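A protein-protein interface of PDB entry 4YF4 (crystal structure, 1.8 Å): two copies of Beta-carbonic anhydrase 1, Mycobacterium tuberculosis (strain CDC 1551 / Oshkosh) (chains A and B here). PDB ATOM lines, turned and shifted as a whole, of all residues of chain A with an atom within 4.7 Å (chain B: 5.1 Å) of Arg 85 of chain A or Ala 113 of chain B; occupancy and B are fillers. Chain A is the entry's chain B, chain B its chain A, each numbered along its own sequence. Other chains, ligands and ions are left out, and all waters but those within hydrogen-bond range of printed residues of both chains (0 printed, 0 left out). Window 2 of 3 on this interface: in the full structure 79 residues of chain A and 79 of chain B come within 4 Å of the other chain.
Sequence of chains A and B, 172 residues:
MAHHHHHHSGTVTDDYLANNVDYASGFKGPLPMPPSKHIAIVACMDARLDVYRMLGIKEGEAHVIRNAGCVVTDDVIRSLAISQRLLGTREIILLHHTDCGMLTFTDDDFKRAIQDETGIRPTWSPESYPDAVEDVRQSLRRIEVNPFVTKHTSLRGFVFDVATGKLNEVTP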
ATOM      1  N   LEU A  80     -24.241   7.174 -20.375  1.00  0.00           N
ATOM      2  CA  LEU A  80     -23.192   6.158 -20.216  1.00  0.00           C
ATOM      3  C   LEU A  80     -21.824   6.703 -20.630  1.00  0.00           C
ATOM      4  O   LEU A  80     -20.814   6.435 -19.965  1.00  0.00           O
ATOM      5  CB  LEU A  80     -23.533   4.872 -20.991  1.00  0.00           C
ATOM      6  CG  LEU A  80     -24.731   4.058 -20.468  1.00  0.00           C
ATOM      7  CD1 LEU A  80     -25.176   2.968 -21.457  1.00  0.00           C
ATOM      8  CD2 LEU A  80     -24.450   3.453 -19.083  1.00  0.00           C
ATOM      9  N   ALA A  81     -21.782   7.457 -21.735  1.00  0.00           N
ATOM     10  CA  ALA A  81     -20.528   8.042 -22.203  1.00  0.00           C
ATOM     11  C   ALA A  81     -19.910   8.933 -21.130  1.00  0.00           C
ATOM     12  O   ALA A  81     -18.711   8.898 -20.894  1.00  0.00           O
ATOM     13  CB  ALA A  81     -20.742   8.851 -23.483  1.00  0.00           C
ATOM     14  N   ILE A  82     -20.739   9.751 -20.495  1.00  0.00           N
ATOM     15  CA  ILE A  82     -20.256  10.636 -19.448  1.00  0.00           C
ATOM     16  C   ILE A  82     -19.800   9.819 -18.224  1.00  0.00           C
ATOM     17  O   ILE A  82     -18.736  10.073 -17.651  1.00  0.00           O
ATOM     18  CB  ILE A  82     -21.342  11.669 -19.045  1.00  0.00           C
ATOM     19  CG1 ILE A  82     -21.500  12.713 -20.159  1.00  0.00           C
ATOM     20  CG2 ILE A  82     -20.972  12.336 -17.729  1.00  0.00           C
ATOM     21  CD1 ILE A  82     -22.772  13.541 -20.079  1.00  0.00           C
ATOM     22  N   SER A  83     -20.607   8.833 -17.856  1.00  0.00           N
ATOM     23  CA  SER A  83     -20.348   7.959 -16.713  1.00  0.00           C
ATOM     24  C   SER A  83     -18.983   7.283 -16.840  1.00  0.00           C
ATOM     25  O   SER A  83     -18.205   7.255 -15.882  1.00  0.00           O
ATOM     26  CB  SER A  83     -21.447   6.903 -16.631  1.00  0.00           C
ATOM     27  OG  SER A  83     -21.192   5.940 -15.617  1.00  0.00           O
ATOM     28  N   GLN A  84     -18.700   6.743 -18.028  1.00  0.00           N
ATOM     29  CA  GLN A  84     -17.431   6.062 -18.287  1.00  0.00           C
ATOM     30  C   GLN A  84     -16.267   7.014 -18.486  1.00  0.00           C
ATOM     31  O   GLN A  84     -15.227   6.876 -17.846  1.00  0.00           O
ATOM     32  CB  GLN A  84     -17.536   5.156 -19.519  1.00  0.00           C
ATOM     33  CG  GLN A  84     -18.537   4.051 -19.352  1.00  0.00           C
ATOM     34  CD  GLN A  84     -18.488   3.010 -20.456  1.00  0.00           C
ATOM     35  OE1 GLN A  84     -17.928   3.238 -21.538  1.00  0.00           O
ATOM     36  NE2 GLN A  84     -19.085   1.857 -20.189  1.00  0.00           N
ATOM     37  N   ARG A  85     -16.441   7.990 -19.369  1.00  0.00           N
ATOM     38  CA  ARG A  85     -15.308   8.824 -19.776  1.00  0.00           C
ATOM     39  C   ARG A  85     -14.893   9.842 -18.707  1.00  0.00           C
ATOM     40  O   ARG A  85     -13.706  10.125 -18.533  1.00  0.00           O
ATOM     41  CB  ARG A  85     -15.599   9.524 -21.110  1.00  0.00           C
ATOM     42  CG  ARG A  85     -15.842   8.559 -22.276  1.00  0.00           C
ATOM     43  CD  ARG A  85     -16.108   9.326 -23.560  1.00  0.00           C
ATOM     44  NE  ARG A  85     -15.045  10.296 -23.809  1.00  0.00           N
ATOM     45  CZ  ARG A  85     -13.915  10.009 -24.450  1.00  0.00           C
ATOM     46  NH1 ARG A  85     -13.707   8.782 -24.922  1.00  0.00           N
ATOM     47  NH2 ARG A  85     -12.998  10.955 -24.625  1.00  0.00           N
ATOM     48  N   LEU A  86     -15.869  10.379 -17.987  1.00  0.00           N
ATOM     49  CA  LEU A  86     -15.614  11.419 -16.998  1.00  0.00           C
ATOM     50  C   LEU A  86     -15.481  10.871 -15.579  1.00  0.00           C
ATOM     51  O   LEU A  86     -14.745  11.423 -14.764  1.00  0.00           O
ATOM     52  CB  LEU A  86     -16.745  12.451 -17.029  1.00  0.00           C
ATOM     53  CG  LEU A  86     -16.573  13.657 -17.951  1.00  0.00           C
ATOM     54  CD1 LEU A  86     -17.863  13.959 -18.669  1.00  0.00           C
ATOM     55  CD2 LEU A  86     -16.133  14.869 -17.141  1.00  0.00           C
ATOM     56  N   LEU A  87     -16.213   9.800 -15.280  1.00  0.00           N
ATOM     57  CA  LEU A  87     -16.375   9.360 -13.891  1.00  0.00           C
ATOM     58  C   LEU A  87     -15.962   7.914 -13.653  1.00  0.00           C
ATOM     59  O   LEU A  87     -16.169   7.371 -12.567  1.00  0.00           O
ATOM     60  CB  LEU A  87     -17.807   9.603 -13.416  1.00  0.00           C
ATOM     61  CG  LEU A  87     -18.131  11.100 -13.286  1.00  0.00           C
ATOM     62  CD1 LEU A  87     -19.624  11.358 -13.056  1.00  0.00           C
ATOM     63  CD2 LEU A  87     -17.315  11.719 -12.180  1.00  0.00           C
ATOM     64  N   PHE A 148     -19.422   5.213 -28.668  1.00  0.00           N
ATOM     65  CA  PHE A 148     -19.190   6.184 -27.597  1.00  0.00           C
ATOM     66  C   PHE A 148     -19.232   5.573 -26.211  1.00  0.00           C
ATOM     67  O   PHE A 148     -18.934   6.232 -25.218  1.00  0.00           O
ATOM     68  CB  PHE A 148     -20.204   7.323 -27.707  1.00  0.00           C
ATOM     69  CG  PHE A 148     -20.222   7.944 -29.067  1.00  0.00           C
ATOM     70  CD1 PHE A 148     -21.401   8.059 -29.784  1.00  0.00           C
ATOM     71  CD2 PHE A 148     -19.041   8.366 -29.645  1.00  0.00           C
ATOM     72  CE1 PHE A 148     -21.407   8.616 -31.043  1.00  0.00           C
ATOM     73  CE2 PHE A 148     -19.033   8.931 -30.911  1.00  0.00           C
ATOM     74  CZ  PHE A 148     -20.219   9.058 -31.610  1.00  0.00           C
ATOM     75  N   LYS A 151     -15.853   1.456 -22.930  1.00  0.00           N
ATOM     76  CA  LYS A 151     -14.884   1.257 -21.868  1.00  0.00           C
ATOM     77  C   LYS A 151     -15.232   0.134 -20.891  1.00  0.00           C
ATOM     78  O   LYS A 151     -14.373  -0.328 -20.138  1.00  0.00           O
ATOM     79  CB  LYS A 151     -14.633   2.582 -21.138  1.00  0.00           C
ATOM     80  CG  LYS A 151     -13.849   3.576 -21.999  1.00  0.00           C
ATOM     81  CD  LYS A 151     -13.437   4.813 -21.220  1.00  0.00           C
ATOM     82  CE  LYS A 151     -12.491   5.694 -22.037  1.00  0.00           C
ATOM     83  NZ  LYS A 151     -12.104   6.951 -21.314  1.00  0.00           N
ATOM     84  N   ASP B 108     -18.410  21.328 -26.025  1.00  0.00           N
ATOM     85  CA  ASP B 108     -17.438  21.370 -27.111  1.00  0.00           C
ATOM     86  C   ASP B 108     -16.173  20.579 -26.739  1.00  0.00           C
ATOM     87  O   ASP B 108     -15.643  19.823 -27.554  1.00  0.00           O
ATOM     88  CB  ASP B 108     -17.118  22.818 -27.498  1.00  0.00           C
ATOM     89  CG  ASP B 108     -18.309  23.525 -28.136  1.00  0.00           C
ATOM     90  OD1 ASP B 108     -19.119  22.838 -28.797  1.00  0.00           O
ATOM     91  OD2 ASP B 108     -18.445  24.761 -27.982  1.00  0.00           O
ATOM     92  N   ASP B 109     -15.719  20.718 -25.499  1.00  0.00           N
ATOM     93  CA  ASP B 109     -14.556  19.963 -25.032  1.00  0.00           C
ATOM     94  C   ASP B 109     -14.822  18.464 -24.996  1.00  0.00           C
ATOM     95  O   ASP B 109     -13.967  17.667 -25.386  1.00  0.00           O
ATOM     96  CB  ASP B 109     -14.120  20.435 -23.644  1.00  0.00           C
ATOM     97  CG  ASP B 109     -13.446  21.791 -23.673  1.00  0.00           C
ATOM     98  OD1 ASP B 109     -12.651  22.043 -24.605  1.00  0.00           O
ATOM     99  OD2 ASP B 109     -13.715  22.606 -22.762  1.00  0.00           O
ATOM    100  N   PHE B 110     -16.004  18.083 -24.518  1.00  0.00           N
ATOM    101  CA  PHE B 110     -16.357  16.679 -24.372  1.00  0.00           C
ATOM    102  C   PHE B 110     -16.446  16.039 -25.756  1.00  0.00           C
ATOM    103  O   PHE B 110     -15.918  14.950 -25.980  1.00  0.00           O
ATOM    104  CB  PHE B 110     -17.673  16.541 -23.602  1.00  0.00           C
ATOM    105  CG  PHE B 110     -18.092  15.119 -23.337  1.00  0.00           C
ATOM    106  CD1 PHE B 110     -17.502  14.383 -22.322  1.00  0.00           C
ATOM    107  CD2 PHE B 110     -19.095  14.530 -24.080  1.00  0.00           C
ATOM    108  CE1 PHE B 110     -17.898  13.083 -22.067  1.00  0.00           C
ATOM    109  CE2 PHE B 110     -19.500  13.225 -23.824  1.00  0.00           C
ATOM    110  CZ  PHE B 110     -18.897  12.502 -22.820  1.00  0.00           C
ATOM    111  N   LYS B 111     -17.083  16.740 -26.689  1.00  0.00           N
ATOM    112  CA  LYS B 111     -17.174  16.254 -28.061  1.00  0.00           C
ATOM    113  C   LYS B 111     -15.815  16.166 -28.758  1.00  0.00           C
ATOM    114  O   LYS B 111     -15.572  15.221 -29.506  1.00  0.00           O
ATOM    115  CB  LYS B 111     -18.107  17.125 -28.888  1.00  0.00           C
ATOM    116  CG  LYS B 111     -19.568  16.919 -28.590  1.00  0.00           C
ATOM    117  CD  LYS B 111     -20.375  17.465 -29.750  1.00  0.00           C
ATOM    118  CE  LYS B 111     -21.815  17.053 -29.661  1.00  0.00           C
ATOM    119  NZ  LYS B 111     -22.532  17.275 -30.945  1.00  0.00           N
ATOM    120  N   ARG B 112     -14.951  17.158 -28.540  1.00  0.00           N
ATOM    121  CA  ARG B 112     -13.644  17.173 -29.181  1.00  0.00           C
ATOM    122  C   ARG B 112     -12.818  15.979 -28.718  1.00  0.00           C
ATOM    123  O   ARG B 112     -12.136  15.337 -29.519  1.00  0.00           O
ATOM    124  CB  ARG B 112     -12.893  18.483 -28.895  1.00  0.00           C
ATOM    125  CG  ARG B 112     -11.601  18.631 -29.704  1.00  0.00           C
ATOM    126  CD  ARG B 112     -10.390  18.912 -28.825  1.00  0.00           C
ATOM    127  NE  ARG B 112      -9.141  18.848 -29.588  1.00  0.00           N
ATOM    128  CZ  ARG B 112      -7.928  19.026 -29.068  1.00  0.00           C
ATOM    129  NH1 ARG B 112      -7.786  19.288 -27.774  1.00  0.00           N
ATOM    130  NH2 ARG B 112      -6.855  18.943 -29.843  1.00  0.00           N
ATOM    131  N   ALA B 113     -12.909  15.680 -27.425  1.00  0.00           N
ATOM    132  CA  ALA B 113     -12.191  14.559 -26.830  1.00  0.00           C
ATOM    133  C   ALA B 113     -12.640  13.234 -27.433  1.00  0.00           C
ATOM    134  O   ALA B 113     -11.817  12.401 -27.802  1.00  0.00           O
ATOM    135  CB  ALA B 113     -12.393  14.545 -25.321  1.00  0.00           C
ATOM    136  N   ILE B 114     -13.953  13.040 -27.517  1.00  0.00           N
ATOM    137  CA  ILE B 114     -14.497  11.851 -28.154  1.00  0.00           C
ATOM    138  C   ILE B 114     -14.065  11.769 -29.616  1.00  0.00           C
ATOM    139  O   ILE B 114     -13.717  10.697 -30.112  1.00  0.00           O
ATOM    140  CB  ILE B 114     -16.040  11.809 -28.058  1.00  0.00           C
ATOM    141  CG1 ILE B 114     -16.468  11.612 -26.610  1.00  0.00           C
ATOM    142  CG2 ILE B 114     -16.605  10.693 -28.922  1.00  0.00           C
ATOM    143  CD1 ILE B 114     -17.970  11.609 -26.415  1.00  0.00           C
ATOM    144  N   GLN B 115     -14.077  12.905 -30.308  1.00  0.00           N
ATOM    145  CA  GLN B 115     -13.715  12.892 -31.718  1.00  0.00           C
ATOM    146  C   GLN B 115     -12.265  12.442 -31.903  1.00  0.00           C
ATOM    147  O   GLN B 115     -11.975  11.628 -32.778  1.00  0.00           O
ATOM    148  CB  GLN B 115     -13.954  14.253 -32.389  1.00  0.00           C
ATOM    149  CG  GLN B 115     -13.567  14.260 -33.870  1.00  0.00           C
ATOM    150  CD  GLN B 115     -13.957  15.540 -34.573  1.00  0.00           C
ATOM    151  OE1 GLN B 115     -14.752  16.322 -34.058  1.00  0.00           O
ATOM    152  NE2 GLN B 115     -13.388  15.769 -35.757  1.00  0.00           N
ATOM    153  N   ASP B 116     -11.368  12.952 -31.062  1.00  0.00           N
ATOM    154  CA  ASP B 116      -9.958  12.562 -31.127  1.00  0.00           C
ATOM    155  C   ASP B 116      -9.753  11.053 -30.974  1.00  0.00           C
ATOM    156  O   ASP B 116      -8.956  10.448 -31.695  1.00  0.00           O
ATOM    157  CB  ASP B 116      -9.138  13.302 -30.065  1.00  0.00           C
ATOM    158  CG  ASP B 116      -9.090  14.796 -30.302  1.00  0.00           C
ATOM    159  OD1 ASP B 116      -9.370  15.234 -31.438  1.00  0.00           O
ATOM    160  OD2 ASP B 116      -8.765  15.534 -29.350  1.00  0.00           O
ATOM    161  N   GLU B 117     -10.474  10.444 -30.038  1.00  0.00           N
ATOM    162  CA  GLU B 117     -10.325   9.014 -29.779  1.00  0.00           C
ATOM    163  C   GLU B 117     -10.978   8.138 -30.841  1.00  0.00           C
ATOM    164  O   GLU B 117     -10.410   7.122 -31.250  1.00  0.00           O
ATOM    165  CB  GLU B 117     -10.895   8.653 -28.411  1.00  0.00           C
ATOM    166  CG  GLU B 117     -10.297   9.433 -27.265  1.00  0.00           C
ATOM    167  CD  GLU B 117     -10.678   8.844 -25.931  1.00  0.00           C
ATOM    168  OE1 GLU B 117     -11.251   7.732 -25.920  1.00  0.00           O
ATOM    169  OE2 GLU B 117     -10.407   9.490 -24.896  1.00  0.00           O
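The backbone carbonyl oxygen of Ile 82 of chain A lies within hydrogen-bond range of the backbone NH of Leu 87 of chain A, at 3.5 Å.
CG1 of Ile 82 of chain A touches CZ of Phe 110 of chain B, at 3.7 Å.
Arg 85 of chain A touches Ala 113 of chain B (NH2 to C, 3.6 Å).
Arg 85 of chain A touches Ile 114 of chain B.
Leu 86 of chain A touches Phe 110 of chain B.
Phe 148 of chain A touches Ile 114 of chain B (CD2 to CG2, 3.4 Å).
Of the 10 printed residues of chain A, 4 touch a printed residue of chain B.
Of the 10 printed residues of chain B, 4 touch a printed residue of chain A.
Printed residues of chain B that touch a printed residue of chain A: Phe 110, Ala 113, Ile 114 and Glu 117.
Among the printed residues, 6 pairs touch across the chains.
No position is printed for both chains.
Of the 6 pairs that touch across the chains among the printed residues, none has its exchanged pair printed and touching as well.
OE1 of Glu 117 of chain B lies within salt-bridge range of NH1 of Arg 85 of chain A (2.9 Å).
Gln 84 of chain A touches none of the printed residues of chain B.
Of chain B, only Ala 113, Ile 114 and Glu 117 come within 4 Å of Arg 85 of chain A.
Of the printed residues of chain B, Phe 148 of chain A touches Ile 114.
Printed residues of chain A within 4 Å of Phe 110 of chain B: Ile 82 (3.7 Å) and Leu 86 (3.5 Å).
Ala 113 of chain B touches one residue of chain A.
Of the printed residues of chain A, Ile 114 of chain B touches Arg 85 (3.4 Å) and Phe 148 (3.4 Å).
The nearest printed residue of chain A that does not touch Phe 110 of chain B is Ala 81 of chain A (4.1 Å).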
